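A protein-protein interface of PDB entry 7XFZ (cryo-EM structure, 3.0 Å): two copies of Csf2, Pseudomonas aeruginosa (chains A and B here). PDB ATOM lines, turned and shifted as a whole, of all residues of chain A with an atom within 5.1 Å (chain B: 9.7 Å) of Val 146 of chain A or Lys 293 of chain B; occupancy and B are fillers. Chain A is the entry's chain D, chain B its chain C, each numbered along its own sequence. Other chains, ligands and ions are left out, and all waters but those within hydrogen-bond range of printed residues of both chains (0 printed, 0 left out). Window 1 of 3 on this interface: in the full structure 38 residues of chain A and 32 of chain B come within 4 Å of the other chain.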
ATOM      1  N   GLY A  67     -13.704 -30.435  18.101  1.00  0.00           N
ATOM      2  CA  GLY A  67     -13.664 -29.499  16.992  1.00  0.00           C
ATOM      3  C   GLY A  67     -12.520 -29.723  16.029  1.00  0.00           C
ATOM      4  O   GLY A  67     -12.610 -29.306  14.870  1.00  0.00           O
ATOM      5  N   MET A  70     -13.873 -32.115  13.390  1.00  0.00           N
ATOM      6  CA  MET A  70     -14.794 -31.409  12.501  1.00  0.00           C
ATOM      7  C   MET A  70     -14.051 -30.492  11.539  1.00  0.00           C
ATOM      8  O   MET A  70     -14.400 -30.414  10.354  1.00  0.00           O
ATOM      9  CB  MET A  70     -15.816 -30.616  13.314  1.00  0.00           C
ATOM     10  CG  MET A  70     -16.279 -31.297  14.581  1.00  0.00           C
ATOM     11  SD  MET A  70     -17.057 -32.884  14.238  1.00  0.00           S
ATOM     12  CE  MET A  70     -18.425 -32.380  13.198  1.00  0.00           C
ATOM     13  N   ARG A  71     -13.036 -29.778  12.026  1.00  0.00           N
ATOM     14  CA  ARG A  71     -12.257 -28.916  11.145  1.00  0.00           C
ATOM     15  C   ARG A  71     -11.545 -29.732  10.073  1.00  0.00           C
ATOM     16  O   ARG A  71     -11.517 -29.343   8.898  1.00  0.00           O
ATOM     17  CB  ARG A  71     -11.260 -28.102  11.968  1.00  0.00           C
ATOM     18  CG  ARG A  71     -10.218 -27.365  11.158  1.00  0.00           C
ATOM     19  CD  ARG A  71      -9.651 -26.201  11.945  1.00  0.00           C
ATOM     20  NE  ARG A  71      -8.630 -25.477  11.200  1.00  0.00           N
ATOM     21  CZ  ARG A  71      -8.591 -24.159  11.069  1.00  0.00           C
ATOM     22  NH1 ARG A  71      -9.511 -23.385  11.618  1.00  0.00           N
ATOM     23  NH2 ARG A  71      -7.607 -23.604  10.371  1.00  0.00           N
ATOM     24  N   LEU A  74     -14.160 -30.848   7.476  1.00  0.00           N
ATOM     25  CA  LEU A  74     -14.440 -29.737   6.573  1.00  0.00           C
ATOM     26  C   LEU A  74     -13.332 -29.574   5.545  1.00  0.00           C
ATOM     27  O   LEU A  74     -13.597 -29.470   4.339  1.00  0.00           O
ATOM     28  CB  LEU A  74     -14.609 -28.448   7.377  1.00  0.00           C
ATOM     29  CG  LEU A  74     -14.936 -27.162   6.614  1.00  0.00           C
ATOM     30  CD1 LEU A  74     -16.353 -27.176   6.076  1.00  0.00           C
ATOM     31  CD2 LEU A  74     -14.711 -25.944   7.499  1.00  0.00           C
ATOM     32  N   LEU A 144     -10.459 -18.943   9.797  1.00  0.00           N
ATOM     33  CA  LEU A 144     -11.569 -19.853  10.027  1.00  0.00           C
ATOM     34  C   LEU A 144     -11.495 -20.405  11.443  1.00  0.00           C
ATOM     35  O   LEU A 144     -10.432 -20.841  11.893  1.00  0.00           O
ATOM     36  CB  LEU A 144     -11.557 -21.000   9.015  1.00  0.00           C
ATOM     37  CG  LEU A 144     -12.663 -22.041   9.179  1.00  0.00           C
ATOM     38  CD1 LEU A 144     -13.961 -21.545   8.575  1.00  0.00           C
ATOM     39  CD2 LEU A 144     -12.246 -23.346   8.547  1.00  0.00           C
ATOM     40  N   MET A 145     -12.628 -20.380  12.142  1.00  0.00           N
ATOM     41  CA  MET A 145     -12.726 -20.865  13.513  1.00  0.00           C
ATOM     42  C   MET A 145     -13.806 -21.934  13.556  1.00  0.00           C
ATOM     43  O   MET A 145     -14.961 -21.661  13.216  1.00  0.00           O
ATOM     44  CB  MET A 145     -13.073 -19.731  14.475  1.00  0.00           C
ATOM     45  CG  MET A 145     -12.026 -18.650  14.585  1.00  0.00           C
ATOM     46  SD  MET A 145     -12.813 -17.062  14.906  1.00  0.00           S
ATOM     47  CE  MET A 145     -12.018 -16.027  13.688  1.00  0.00           C
ATOM     48  N   VAL A 146     -13.441 -23.139  13.980  1.00  0.00           N
ATOM     49  CA  VAL A 146     -14.365 -24.267  14.015  1.00  0.00           C
ATOM     50  C   VAL A 146     -14.541 -24.700  15.462  1.00  0.00           C
ATOM     51  O   VAL A 146     -13.568 -25.075  16.126  1.00  0.00           O
ATOM     52  CB  VAL A 146     -13.874 -25.438  13.152  1.00  0.00           C
ATOM     53  CG1 VAL A 146     -14.848 -26.593  13.239  1.00  0.00           C
ATOM     54  CG2 VAL A 146     -13.705 -24.997  11.713  1.00  0.00           C
ATOM     55  N   ASP A 147     -15.779 -24.660  15.939  1.00  0.00           N
ATOM     56  CA  ASP A 147     -16.126 -25.101  17.278  1.00  0.00           C
ATOM     57  C   ASP A 147     -16.361 -26.612  17.256  1.00  0.00           C
ATOM     58  O   ASP A 147     -16.177 -27.273  16.232  1.00  0.00           O
ATOM     59  CB  ASP A 147     -17.345 -24.325  17.775  1.00  0.00           C
ATOM     60  CG  ASP A 147     -17.501 -24.374  19.279  1.00  0.00           C
ATOM     61  OD1 ASP A 147     -16.612 -24.932  19.954  1.00  0.00           O
ATOM     62  OD2 ASP A 147     -18.519 -23.859  19.785  1.00  0.00           O
ATOM     63  N   SER A 148     -16.771 -27.179  18.385  1.00  0.00           N
ATOM     64  CA  SER A 148     -17.080 -28.596  18.475  1.00  0.00           C
ATOM     65  C   SER A 148     -18.576 -28.818  18.294  1.00  0.00           C
ATOM     66  O   SER A 148     -19.368 -27.874  18.251  1.00  0.00           O
ATOM     67  CB  SER A 148     -16.617 -29.180  19.813  1.00  0.00           C
ATOM     68  OG  SER A 148     -17.196 -28.489  20.900  1.00  0.00           O
ATOM     69  N   TRP A 260     -23.777 -26.994  15.524  1.00  0.00           N
ATOM     70  CA  TRP A 260     -22.398 -26.751  15.127  1.00  0.00           C
ATOM     71  C   TRP A 260     -22.220 -25.287  14.758  1.00  0.00           C
ATOM     72  O   TRP A 260     -22.979 -24.746  13.951  1.00  0.00           O
ATOM     73  CB  TRP A 260     -22.010 -27.642  13.946  1.00  0.00           C
ATOM     74  CG  TRP A 260     -20.554 -27.650  13.646  1.00  0.00           C
ATOM     75  CD1 TRP A 260     -19.543 -27.287  14.482  1.00  0.00           C
ATOM     76  CD2 TRP A 260     -19.939 -28.043  12.417  1.00  0.00           C
ATOM     77  NE1 TRP A 260     -18.334 -27.427  13.850  1.00  0.00           N
ATOM     78  CE2 TRP A 260     -18.549 -27.891  12.580  1.00  0.00           C
ATOM     79  CE3 TRP A 260     -20.429 -28.510  11.194  1.00  0.00           C
ATOM     80  CZ2 TRP A 260     -17.642 -28.188  11.566  1.00  0.00           C
ATOM     81  CZ3 TRP A 260     -19.528 -28.805  10.188  1.00  0.00           C
ATOM     82  CH2 TRP A 260     -18.150 -28.643  10.380  1.00  0.00           C
ATOM     83  N   ARG A 261     -21.207 -24.651  15.342  1.00  0.00           N
ATOM     84  CA  ARG A 261     -20.951 -23.230  15.154  1.00  0.00           C
ATOM     85  C   ARG A 261     -19.617 -23.038  14.446  1.00  0.00           C
ATOM     86  O   ARG A 261     -18.603 -23.608  14.858  1.00  0.00           O
ATOM     87  CB  ARG A 261     -20.947 -22.495  16.494  1.00  0.00           C
ATOM     88  CG  ARG A 261     -22.306 -22.426  17.160  1.00  0.00           C
ATOM     89  CD  ARG A 261     -22.280 -21.519  18.375  1.00  0.00           C
ATOM     90  NE  ARG A 261     -21.577 -22.131  19.495  1.00  0.00           N
ATOM     91  CZ  ARG A 261     -21.975 -22.062  20.758  1.00  0.00           C
ATOM     92  NH1 ARG A 261     -23.078 -21.416  21.100  1.00  0.00           N
ATOM     93  NH2 ARG A 261     -21.249 -22.656  21.701  1.00  0.00           N
ATOM     94  N   ILE A 262     -19.625 -22.240  13.381  1.00  0.00           N
ATOM     95  CA  ILE A 262     -18.428 -21.899  12.623  1.00  0.00           C
ATOM     96  C   ILE A 262     -18.390 -20.388  12.445  1.00  0.00           C
ATOM     97  O   ILE A 262     -19.426 -19.756  12.220  1.00  0.00           O
ATOM     98  CB  ILE A 262     -18.392 -22.606  11.251  1.00  0.00           C
ATOM     99  CG1 ILE A 262     -18.796 -24.075  11.386  1.00  0.00           C
ATOM    100  CG2 ILE A 262     -17.018 -22.484  10.617  1.00  0.00           C
ATOM    101  CD1 ILE A 262     -20.090 -24.418  10.688  1.00  0.00           C
ATOM    102  N   ILE B  10     -18.583 -18.877  26.447  1.00  0.00           N
ATOM    103  CA  ILE B  10     -19.335 -19.968  25.839  1.00  0.00           C
ATOM    104  C   ILE B  10     -18.433 -21.089  25.337  1.00  0.00           C
ATOM    105  O   ILE B  10     -18.892 -22.233  25.213  1.00  0.00           O
ATOM    106  CB  ILE B  10     -20.195 -19.444  24.675  1.00  0.00           C
ATOM    107  CG1 ILE B  10     -20.859 -18.123  25.051  1.00  0.00           C
ATOM    108  CG2 ILE B  10     -21.255 -20.453  24.292  1.00  0.00           C
ATOM    109  CD1 ILE B  10     -21.692 -17.546  23.937  1.00  0.00           C
ATOM    110  N   THR B  11     -17.173 -20.798  25.050  1.00  0.00           N
ATOM    111  CA  THR B  11     -16.184 -21.759  24.601  1.00  0.00           C
ATOM    112  C   THR B  11     -15.037 -21.802  25.603  1.00  0.00           C
ATOM    113  O   THR B  11     -14.872 -20.875  26.404  1.00  0.00           O
ATOM    114  CB  THR B  11     -15.653 -21.389  23.209  1.00  0.00           C
ATOM    115  OG1 THR B  11     -15.081 -20.079  23.245  1.00  0.00           O
ATOM    116  CG2 THR B  11     -16.771 -21.414  22.187  1.00  0.00           C
ATOM    117  N   PRO B  12     -14.237 -22.869  25.605  1.00  0.00           N
ATOM    118  CA  PRO B  12     -13.128 -22.949  26.562  1.00  0.00           C
ATOM    119  C   PRO B  12     -12.146 -21.800  26.397  1.00  0.00           C
ATOM    120  O   PRO B  12     -11.946 -21.280  25.299  1.00  0.00           O
ATOM    121  CB  PRO B  12     -12.478 -24.295  26.232  1.00  0.00           C
ATOM    122  CG  PRO B  12     -13.563 -25.096  25.639  1.00  0.00           C
ATOM    123  CD  PRO B  12     -14.421 -24.137  24.877  1.00  0.00           C
ATOM    124  N   ILE B  13     -11.541 -21.399  27.511  1.00  0.00           N
ATOM    125  CA  ILE B  13     -10.550 -20.330  27.539  1.00  0.00           C
ATOM    126  C   ILE B  13      -9.180 -20.956  27.752  1.00  0.00           C
ATOM    127  O   ILE B  13      -8.990 -21.750  28.681  1.00  0.00           O
ATOM    128  CB  ILE B  13     -10.874 -19.303  28.638  1.00  0.00           C
ATOM    129  CG1 ILE B  13     -11.912 -18.301  28.135  1.00  0.00           C
ATOM    130  CG2 ILE B  13      -9.621 -18.577  29.086  1.00  0.00           C
ATOM    131  CD1 ILE B  13     -12.226 -17.207  29.113  1.00  0.00           C
ATOM    132  N   PHE B  14      -8.227 -20.607  26.892  1.00  0.00           N
ATOM    133  CA  PHE B  14      -6.900 -21.213  26.904  1.00  0.00           C
ATOM    134  C   PHE B  14      -5.851 -20.114  26.817  1.00  0.00           C
ATOM    135  O   PHE B  14      -5.628 -19.547  25.744  1.00  0.00           O
ATOM    136  CB  PHE B  14      -6.749 -22.207  25.752  1.00  0.00           C
ATOM    137  CG  PHE B  14      -5.375 -22.792  25.628  1.00  0.00           C
ATOM    138  CD1 PHE B  14      -4.823 -23.514  26.667  1.00  0.00           C
ATOM    139  CD2 PHE B  14      -4.644 -22.632  24.469  1.00  0.00           C
ATOM    140  CE1 PHE B  14      -3.566 -24.055  26.558  1.00  0.00           C
ATOM    141  CE2 PHE B  14      -3.385 -23.173  24.353  1.00  0.00           C
ATOM    142  CZ  PHE B  14      -2.846 -23.886  25.401  1.00  0.00           C
ATOM    143  N   VAL B 177      -7.286 -31.955  27.321  1.00  0.00           N
ATOM    144  CA  VAL B 177      -7.786 -32.483  26.057  1.00  0.00           C
ATOM    145  C   VAL B 177      -6.600 -32.895  25.195  1.00  0.00           C
ATOM    146  O   VAL B 177      -5.503 -32.342  25.326  1.00  0.00           O
ATOM    147  CB  VAL B 177      -8.677 -31.459  25.323  1.00  0.00           C
ATOM    148  CG1 VAL B 177      -9.620 -30.779  26.299  1.00  0.00           C
ATOM    149  CG2 VAL B 177      -7.836 -30.429  24.615  1.00  0.00           C
ATOM    150  N   TRP B 178      -6.821 -33.873  24.320  1.00  0.00           N
ATOM    151  CA  TRP B 178      -5.769 -34.465  23.507  1.00  0.00           C
ATOM    152  C   TRP B 178      -5.957 -34.110  22.039  1.00  0.00           C
ATOM    153  O   TRP B 178      -7.084 -33.914  21.576  1.00  0.00           O
ATOM    154  CB  TRP B 178      -5.746 -35.985  23.667  1.00  0.00           C
ATOM    155  CG  TRP B 178      -5.332 -36.442  25.026  1.00  0.00           C
ATOM    156  CD1 TRP B 178      -6.105 -36.497  26.144  1.00  0.00           C
ATOM    157  CD2 TRP B 178      -4.038 -36.913  25.408  1.00  0.00           C
ATOM    158  NE1 TRP B 178      -5.372 -36.972  27.201  1.00  0.00           N
ATOM    159  CE2 TRP B 178      -4.099 -37.236  26.775  1.00  0.00           C
ATOM    160  CE3 TRP B 178      -2.833 -37.095  24.726  1.00  0.00           C
ATOM    161  CZ2 TRP B 178      -3.003 -37.729  27.472  1.00  0.00           C
ATOM    162  CZ3 TRP B 178      -1.747 -37.582  25.419  1.00  0.00           C
ATOM    163  CH2 TRP B 178      -1.838 -37.894  26.778  1.00  0.00           C
ATOM    164  N   ALA B 179      -4.846 -34.032  21.311  1.00  0.00           N
ATOM    165  CA  ALA B 179      -4.855 -33.719  19.890  1.00  0.00           C
ATOM    166  C   ALA B 179      -3.899 -34.647  19.154  1.00  0.00           C
ATOM    167  O   ALA B 179      -2.989 -35.229  19.743  1.00  0.00           O
ATOM    168  CB  ALA B 179      -4.474 -32.258  19.633  1.00  0.00           C
ATOM    169  N   ARG B 180      -4.119 -34.776  17.846  1.00  0.00           N
ATOM    170  CA  ARG B 180      -3.347 -35.681  17.008  1.00  0.00           C
ATOM    171  C   ARG B 180      -3.026 -35.001  15.686  1.00  0.00           C
ATOM    172  O   ARG B 180      -3.670 -34.026  15.295  1.00  0.00           O
ATOM    173  CB  ARG B 180      -4.109 -36.989  16.755  1.00  0.00           C
ATOM    174  CG  ARG B 180      -3.233 -38.185  16.471  1.00  0.00           C
ATOM    175  CD  ARG B 180      -4.031 -39.474  16.500  1.00  0.00           C
ATOM    176  NE  ARG B 180      -5.211 -39.425  15.645  1.00  0.00           N
ATOM    177  CZ  ARG B 180      -5.797 -40.493  15.122  1.00  0.00           C
ATOM    178  NH1 ARG B 180      -5.329 -41.711  15.333  1.00  0.00           N
ATOM    179  NH2 ARG B 180      -6.881 -40.335  14.369  1.00  0.00           N
ATOM    180  N   ASN B 247      -0.196 -35.061  21.422  1.00  0.00           N
ATOM    181  CA  ASN B 247       0.086 -34.171  22.539  1.00  0.00           C
ATOM    182  C   ASN B 247      -1.231 -33.722  23.160  1.00  0.00           C
ATOM    183  O   ASN B 247      -2.313 -34.022  22.653  1.00  0.00           O
ATOM    184  CB  ASN B 247       0.941 -32.989  22.082  1.00  0.00           C
ATOM    185  CG  ASN B 247       0.415 -32.345  20.817  1.00  0.00           C
ATOM    186  OD1 ASN B 247      -0.668 -31.767  20.802  1.00  0.00           O
ATOM    187  ND2 ASN B 247       1.185 -32.444  19.743  1.00  0.00           N
ATOM    188  N   ALA B 248      -1.131 -32.996  24.273  1.00  0.00           N
ATOM    189  CA  ALA B 248      -2.305 -32.586  25.028  1.00  0.00           C
ATOM    190  C   ALA B 248      -2.127 -31.162  25.528  1.00  0.00           C
ATOM    191  O   ALA B 248      -1.011 -30.645  25.607  1.00  0.00           O
ATOM    192  CB  ALA B 248      -2.567 -33.528  26.207  1.00  0.00           C
ATOM    193  N   HIS B 249      -3.248 -30.528  25.863  1.00  0.00           N
ATOM    194  CA  HIS B 249      -3.225 -29.212  26.484  1.00  0.00           C
ATOM    195  C   HIS B 249      -4.428 -29.066  27.404  1.00  0.00           C
ATOM    196  O   HIS B 249      -5.397 -29.821  27.320  1.00  0.00           O
ATOM    197  CB  HIS B 249      -3.192 -28.081  25.449  1.00  0.00           C
ATOM    198  CG  HIS B 249      -4.446 -27.952  24.642  1.00  0.00           C
ATOM    199  ND1 HIS B 249      -5.303 -26.880  24.770  1.00  0.00           N
ATOM    200  CD2 HIS B 249      -4.965 -28.734  23.668  1.00  0.00           C
ATOM    201  CE1 HIS B 249      -6.309 -27.020  23.926  1.00  0.00           C
ATOM    202  NE2 HIS B 249      -6.126 -28.135  23.242  1.00  0.00           N
ATOM    203  N   GLU B 250      -4.345 -28.078  28.290  1.00  0.00           N
ATOM    204  CA  GLU B 250      -5.316 -27.870  29.354  1.00  0.00           C
ATOM    205  C   GLU B 250      -6.087 -26.578  29.122  1.00  0.00           C
ATOM    206  O   GLU B 250      -5.492 -25.533  28.847  1.00  0.00           O
ATOM    207  CB  GLU B 250      -4.613 -27.819  30.710  1.00  0.00           C
ATOM    208  CG  GLU B 250      -5.476 -28.219  31.880  1.00  0.00           C
ATOM    209  CD  GLU B 250      -4.837 -27.873  33.206  1.00  0.00           C
ATOM    210  OE1 GLU B 250      -3.747 -28.405  33.500  1.00  0.00           O
ATOM    211  OE2 GLU B 250      -5.422 -27.065  33.954  1.00  0.00           O
ATOM    212  N   VAL B 251      -7.412 -26.646  29.251  1.00  0.00           N
ATOM    213  CA  VAL B 251      -8.284 -25.502  29.026  1.00  0.00           C
ATOM    214  C   VAL B 251      -9.177 -25.307  30.245  1.00  0.00           C
ATOM    215  O   VAL B 251      -9.234 -26.144  31.143  1.00  0.00           O
ATOM    216  CB  VAL B 251      -9.144 -25.656  27.754  1.00  0.00           C
ATOM    217  CG1 VAL B 251      -8.264 -25.791  26.534  1.00  0.00           C
ATOM    218  CG2 VAL B 251     -10.068 -26.849  27.880  1.00  0.00           C
ATOM    219  N   ARG B 286     -12.161 -12.232  20.736  1.00  0.00           N
ATOM    220  CA  ARG B 286     -11.847 -13.431  21.500  1.00  0.00           C
ATOM    221  C   ARG B 286     -10.836 -13.092  22.584  1.00  0.00           C
ATOM    222  O   ARG B 286     -10.077 -12.129  22.450  1.00  0.00           O
ATOM    223  CB  ARG B 286     -11.297 -14.535  20.593  1.00  0.00           C
ATOM    224  CG  ARG B 286     -12.165 -14.848  19.390  1.00  0.00           C
ATOM    225  CD  ARG B 286     -13.373 -15.673  19.781  1.00  0.00           C
ATOM    226  NE  ARG B 286     -14.256 -15.924  18.650  1.00  0.00           N
ATOM    227  CZ  ARG B 286     -15.362 -15.239  18.397  1.00  0.00           C
ATOM    228  NH1 ARG B 286     -15.754 -14.247  19.178  1.00  0.00           N
ATOM    229  NH2 ARG B 286     -16.094 -15.558  17.336  1.00  0.00           N
ATOM    230  N   GLY B 289      -5.738 -17.136  23.588  1.00  0.00           N
ATOM    231  CA  GLY B 289      -5.410 -17.816  22.350  1.00  0.00           C
ATOM    232  C   GLY B 289      -6.311 -18.979  21.997  1.00  0.00           C
ATOM    233  O   GLY B 289      -7.440 -19.073  22.485  1.00  0.00           O
ATOM    234  N   GLY B 290      -5.813 -19.885  21.159  1.00  0.00           N
ATOM    235  CA  GLY B 290      -6.642 -20.953  20.621  1.00  0.00           C
ATOM    236  C   GLY B 290      -7.500 -20.506  19.459  1.00  0.00           C
ATOM    237  O   GLY B 290      -8.697 -20.813  19.417  1.00  0.00           O
ATOM    238  N   HIS B 291      -6.904 -19.792  18.503  1.00  0.00           N
ATOM    239  CA  HIS B 291      -7.681 -19.126  17.461  1.00  0.00           C
ATOM    240  C   HIS B 291      -8.396 -20.122  16.556  1.00  0.00           C
ATOM    241  O   HIS B 291      -9.576 -19.941  16.235  1.00  0.00           O
ATOM    242  CB  HIS B 291      -6.763 -18.219  16.643  1.00  0.00           C
ATOM    243  CG  HIS B 291      -7.408 -17.645  15.421  1.00  0.00           C
ATOM    244  ND1 HIS B 291      -8.362 -16.654  15.480  1.00  0.00           N
ATOM    245  CD2 HIS B 291      -7.225 -17.913  14.107  1.00  0.00           C
ATOM    246  CE1 HIS B 291      -8.744 -16.341  14.256  1.00  0.00           C
ATOM    247  NE2 HIS B 291      -8.070 -17.091  13.404  1.00  0.00           N
ATOM    248  N   SER B 292      -7.706 -21.184  16.137  1.00  0.00           N
ATOM    249  CA  SER B 292      -8.282 -22.087  15.148  1.00  0.00           C
ATOM    250  C   SER B 292      -9.391 -22.951  15.733  1.00  0.00           C
ATOM    251  O   SER B 292     -10.159 -23.559  14.980  1.00  0.00           O
ATOM    252  CB  SER B 292      -7.190 -22.968  14.542  1.00  0.00           C
ATOM    253  OG  SER B 292      -6.541 -23.735  15.537  1.00  0.00           O
ATOM    254  N   LYS B 293      -9.493 -23.027  17.057  1.00  0.00           N
ATOM    255  CA  LYS B 293     -10.495 -23.852  17.714  1.00  0.00           C
ATOM    256  C   LYS B 293     -11.661 -23.045  18.271  1.00  0.00           C
ATOM    257  O   LYS B 293     -12.483 -23.602  19.005  1.00  0.00           O
ATOM    258  CB  LYS B 293      -9.849 -24.672  18.830  1.00  0.00           C
ATOM    259  CG  LYS B 293      -9.217 -25.967  18.354  1.00  0.00           C
ATOM    260  CD  LYS B 293      -8.261 -26.537  19.385  1.00  0.00           C
ATOM    261  CE  LYS B 293      -6.835 -26.075  19.141  1.00  0.00           C
ATOM    262  NZ  LYS B 293      -6.665 -24.612  19.338  1.00  0.00           N
ATOM    263  N   ASP B 294     -11.749 -21.757  17.940  1.00  0.00           N
ATOM    264  CA  ASP B 294     -12.834 -20.887  18.396  1.00  0.00           C
ATOM    265  C   ASP B 294     -12.876 -20.801  19.922  1.00  0.00           C
ATOM    266  O   ASP B 294     -13.940 -20.827  20.540  1.00  0.00           O
ATOM    267  CB  ASP B 294     -14.181 -21.348  17.831  1.00  0.00           C
ATOM    268  CG  ASP B 294     -15.192 -20.220  17.723  1.00  0.00           C
ATOM    269  OD1 ASP B 294     -14.780 -19.042  17.736  1.00  0.00           O
ATOM    270  OD2 ASP B 294     -16.401 -20.512  17.615  1.00  0.00           O
ATOM    271  N   TYR B 295     -11.699 -20.695  20.530  1.00  0.00           N
ATOM    272  CA  TYR B 295     -11.590 -20.485  21.965  1.00  0.00           C
ATOM    273  C   TYR B 295     -11.686 -19.001  22.287  1.00  0.00           C
ATOM    274  O   TYR B 295     -11.256 -18.148  21.507  1.00  0.00           O
ATOM    275  CB  TYR B 295     -10.270 -21.033  22.509  1.00  0.00           C
ATOM    276  CG  TYR B 295     -10.176 -22.538  22.583  1.00  0.00           C
ATOM    277  CD1 TYR B 295     -11.290 -23.337  22.389  1.00  0.00           C
ATOM    278  CD2 TYR B 295      -8.970 -23.157  22.871  1.00  0.00           C
ATOM    279  CE1 TYR B 295     -11.202 -24.711  22.463  1.00  0.00           C
ATOM    280  CE2 TYR B 295      -8.873 -24.528  22.947  1.00  0.00           C
ATOM    281  CZ  TYR B 295      -9.990 -25.299  22.742  1.00  0.00           C
ATOM    282  OH  TYR B 295      -9.894 -26.666  22.821  1.00  0.00           O
ATOM    283  N   GLY B 296     -12.246 -18.699  23.453  1.00  0.00           N
ATOM    284  CA  GLY B 296     -12.306 -17.336  23.933  1.00  0.00           C
ATOM    285  C   GLY B 296     -13.581 -16.583  23.633  1.00  0.00           C
ATOM    286  O   GLY B 296     -13.603 -15.359  23.792  1.00  0.00           O
ATOM    287  N   ARG B 297     -14.635 -17.263  23.198  1.00  0.00           N
ATOM    288  CA  ARG B 297     -15.912 -16.605  22.967  1.00  0.00           C
ATOM    289  C   ARG B 297     -16.592 -16.287  24.291  1.00  0.00           C
ATOM    290  O   ARG B 297     -16.439 -17.008  25.279  1.00  0.00           O
ATOM    291  CB  ARG B 297     -16.818 -17.487  22.113  1.00  0.00           C
ATOM    292  CG  ARG B 297     -17.702 -16.720  21.160  1.00  0.00           C
ATOM    293  CD  ARG B 297     -18.271 -17.637  20.100  1.00  0.00           C
ATOM    294  NE  ARG B 297     -19.571 -17.184  19.624  1.00  0.00           N
ATOM    295  CZ  ARG B 297     -20.254 -17.771  18.652  1.00  0.00           C
ATOM    296  NH1 ARG B 297     -19.785 -18.835  18.023  1.00  0.00           N
ATOM    297  NH2 ARG B 297     -21.438 -17.276  18.301  1.00  0.00           N
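O of Ser 292 of chain B lies within hydrogen-bond range of NH1 of Arg 71 of chain A (3.4 Å). The backbone carbonyl oxygen (O) of Ser 292 of chain B sits at hydrogen-bond distance from the backbone NH (N) of Val 146 of chain A (3.5 Å). The backbone carbonyl oxygen (O) of Val 146 of chain A lies close to the backbone carbonyl oxygen (O) of Lys 293 of chain B.
The backbone NH (N) of Ile 10 of chain B lies within hydrogen-bond range of the backbone carbonyl oxygen (O) of Arg 297 of chain B (3.1 Å). The side-chain hydroxyl of Thr 11 of chain B lies within hydrogen-bond range of the backbone carbonyl oxygen of Asp 294 of chain B. The side-chain hydroxyl of Thr 11 of chain B lies within hydrogen-bond range of the backbone NH of Gly 296 of chain B, at 3.2 Å. OG1 of Thr 11 of chain B lies within hydrogen-bond range of N of Arg 297 of chain B (2.9 Å). OD2 of Asp 294 of chain B lies within salt-bridge range of NH1 of Arg 297 of chain B. NH1 of Arg 71 of chain A sits at hydrogen-bond distance from O of Leu 144 of chain A, at 2.7 Å.
Among the printed residues, pairs that only touch across the chains: Met 145 of chain A with His 291 of chain B, Met 145 of chain A with Ser 292 of chain B, Met 145 of chain A with Asp 294 of chain B, Asp 147 of chain A with Thr 11 of chain B, Asp 147 of chain A with Asp 294 of chain B, Arg 261 of chain A with Ile 10 of chain B and Arg 261 of chain A with Arg 297 of chain B.
Val 146 of chain A touches just these residues of chain B: Ser 292 (3.5 Å) and Lys 293 (3.4 Å). Of the printed residues of chain B, Arg 261 of chain A touches Ile 10 (3.4 Å) and Arg 297 (3.7 Å). Of the printed residues of chain A, Ile 10 of chain B touches Arg 261. Of the printed residues of chain A, Thr 11 of chain B touches Asp 147 (3.8 Å). Ile 13 of chain B touches none of the printed residues of chain A. Phe 14 of chain B touches none of the printed residues of chain A. Of the printed residues of chain A, His 291 of chain B touches Met 145 (3.2 Å). Of chain A, only Val 146 (3.4 Å) comes within 4 Å of Lys 293 of chain B. The nearest residue of chain B that does not touch Val 146 of chain A is Asp 294 of chain B (4.1 Å). The nearest residue of chain A that does not touch Lys 293 of chain B is Asp 147 of chain A (4.3 Å).
Hydrophobic or aromatic side chains of chain A that line the printed part of chain B: Met 145. Of the 24 printed residues of chain B, 7 touch a printed residue of chain A. Hydrophobic or aromatic side chains of chain B within 4 Å of the printed part of chain A: Ile 10 and His 291. Among the printed residues, 10 pairs touch across the chains. Among the printed residues, no Asp or Glu carboxylate lies within 4 Å of a Lys or Arg side-chain nitrogen of the other chain.
No position is printed for both chains.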
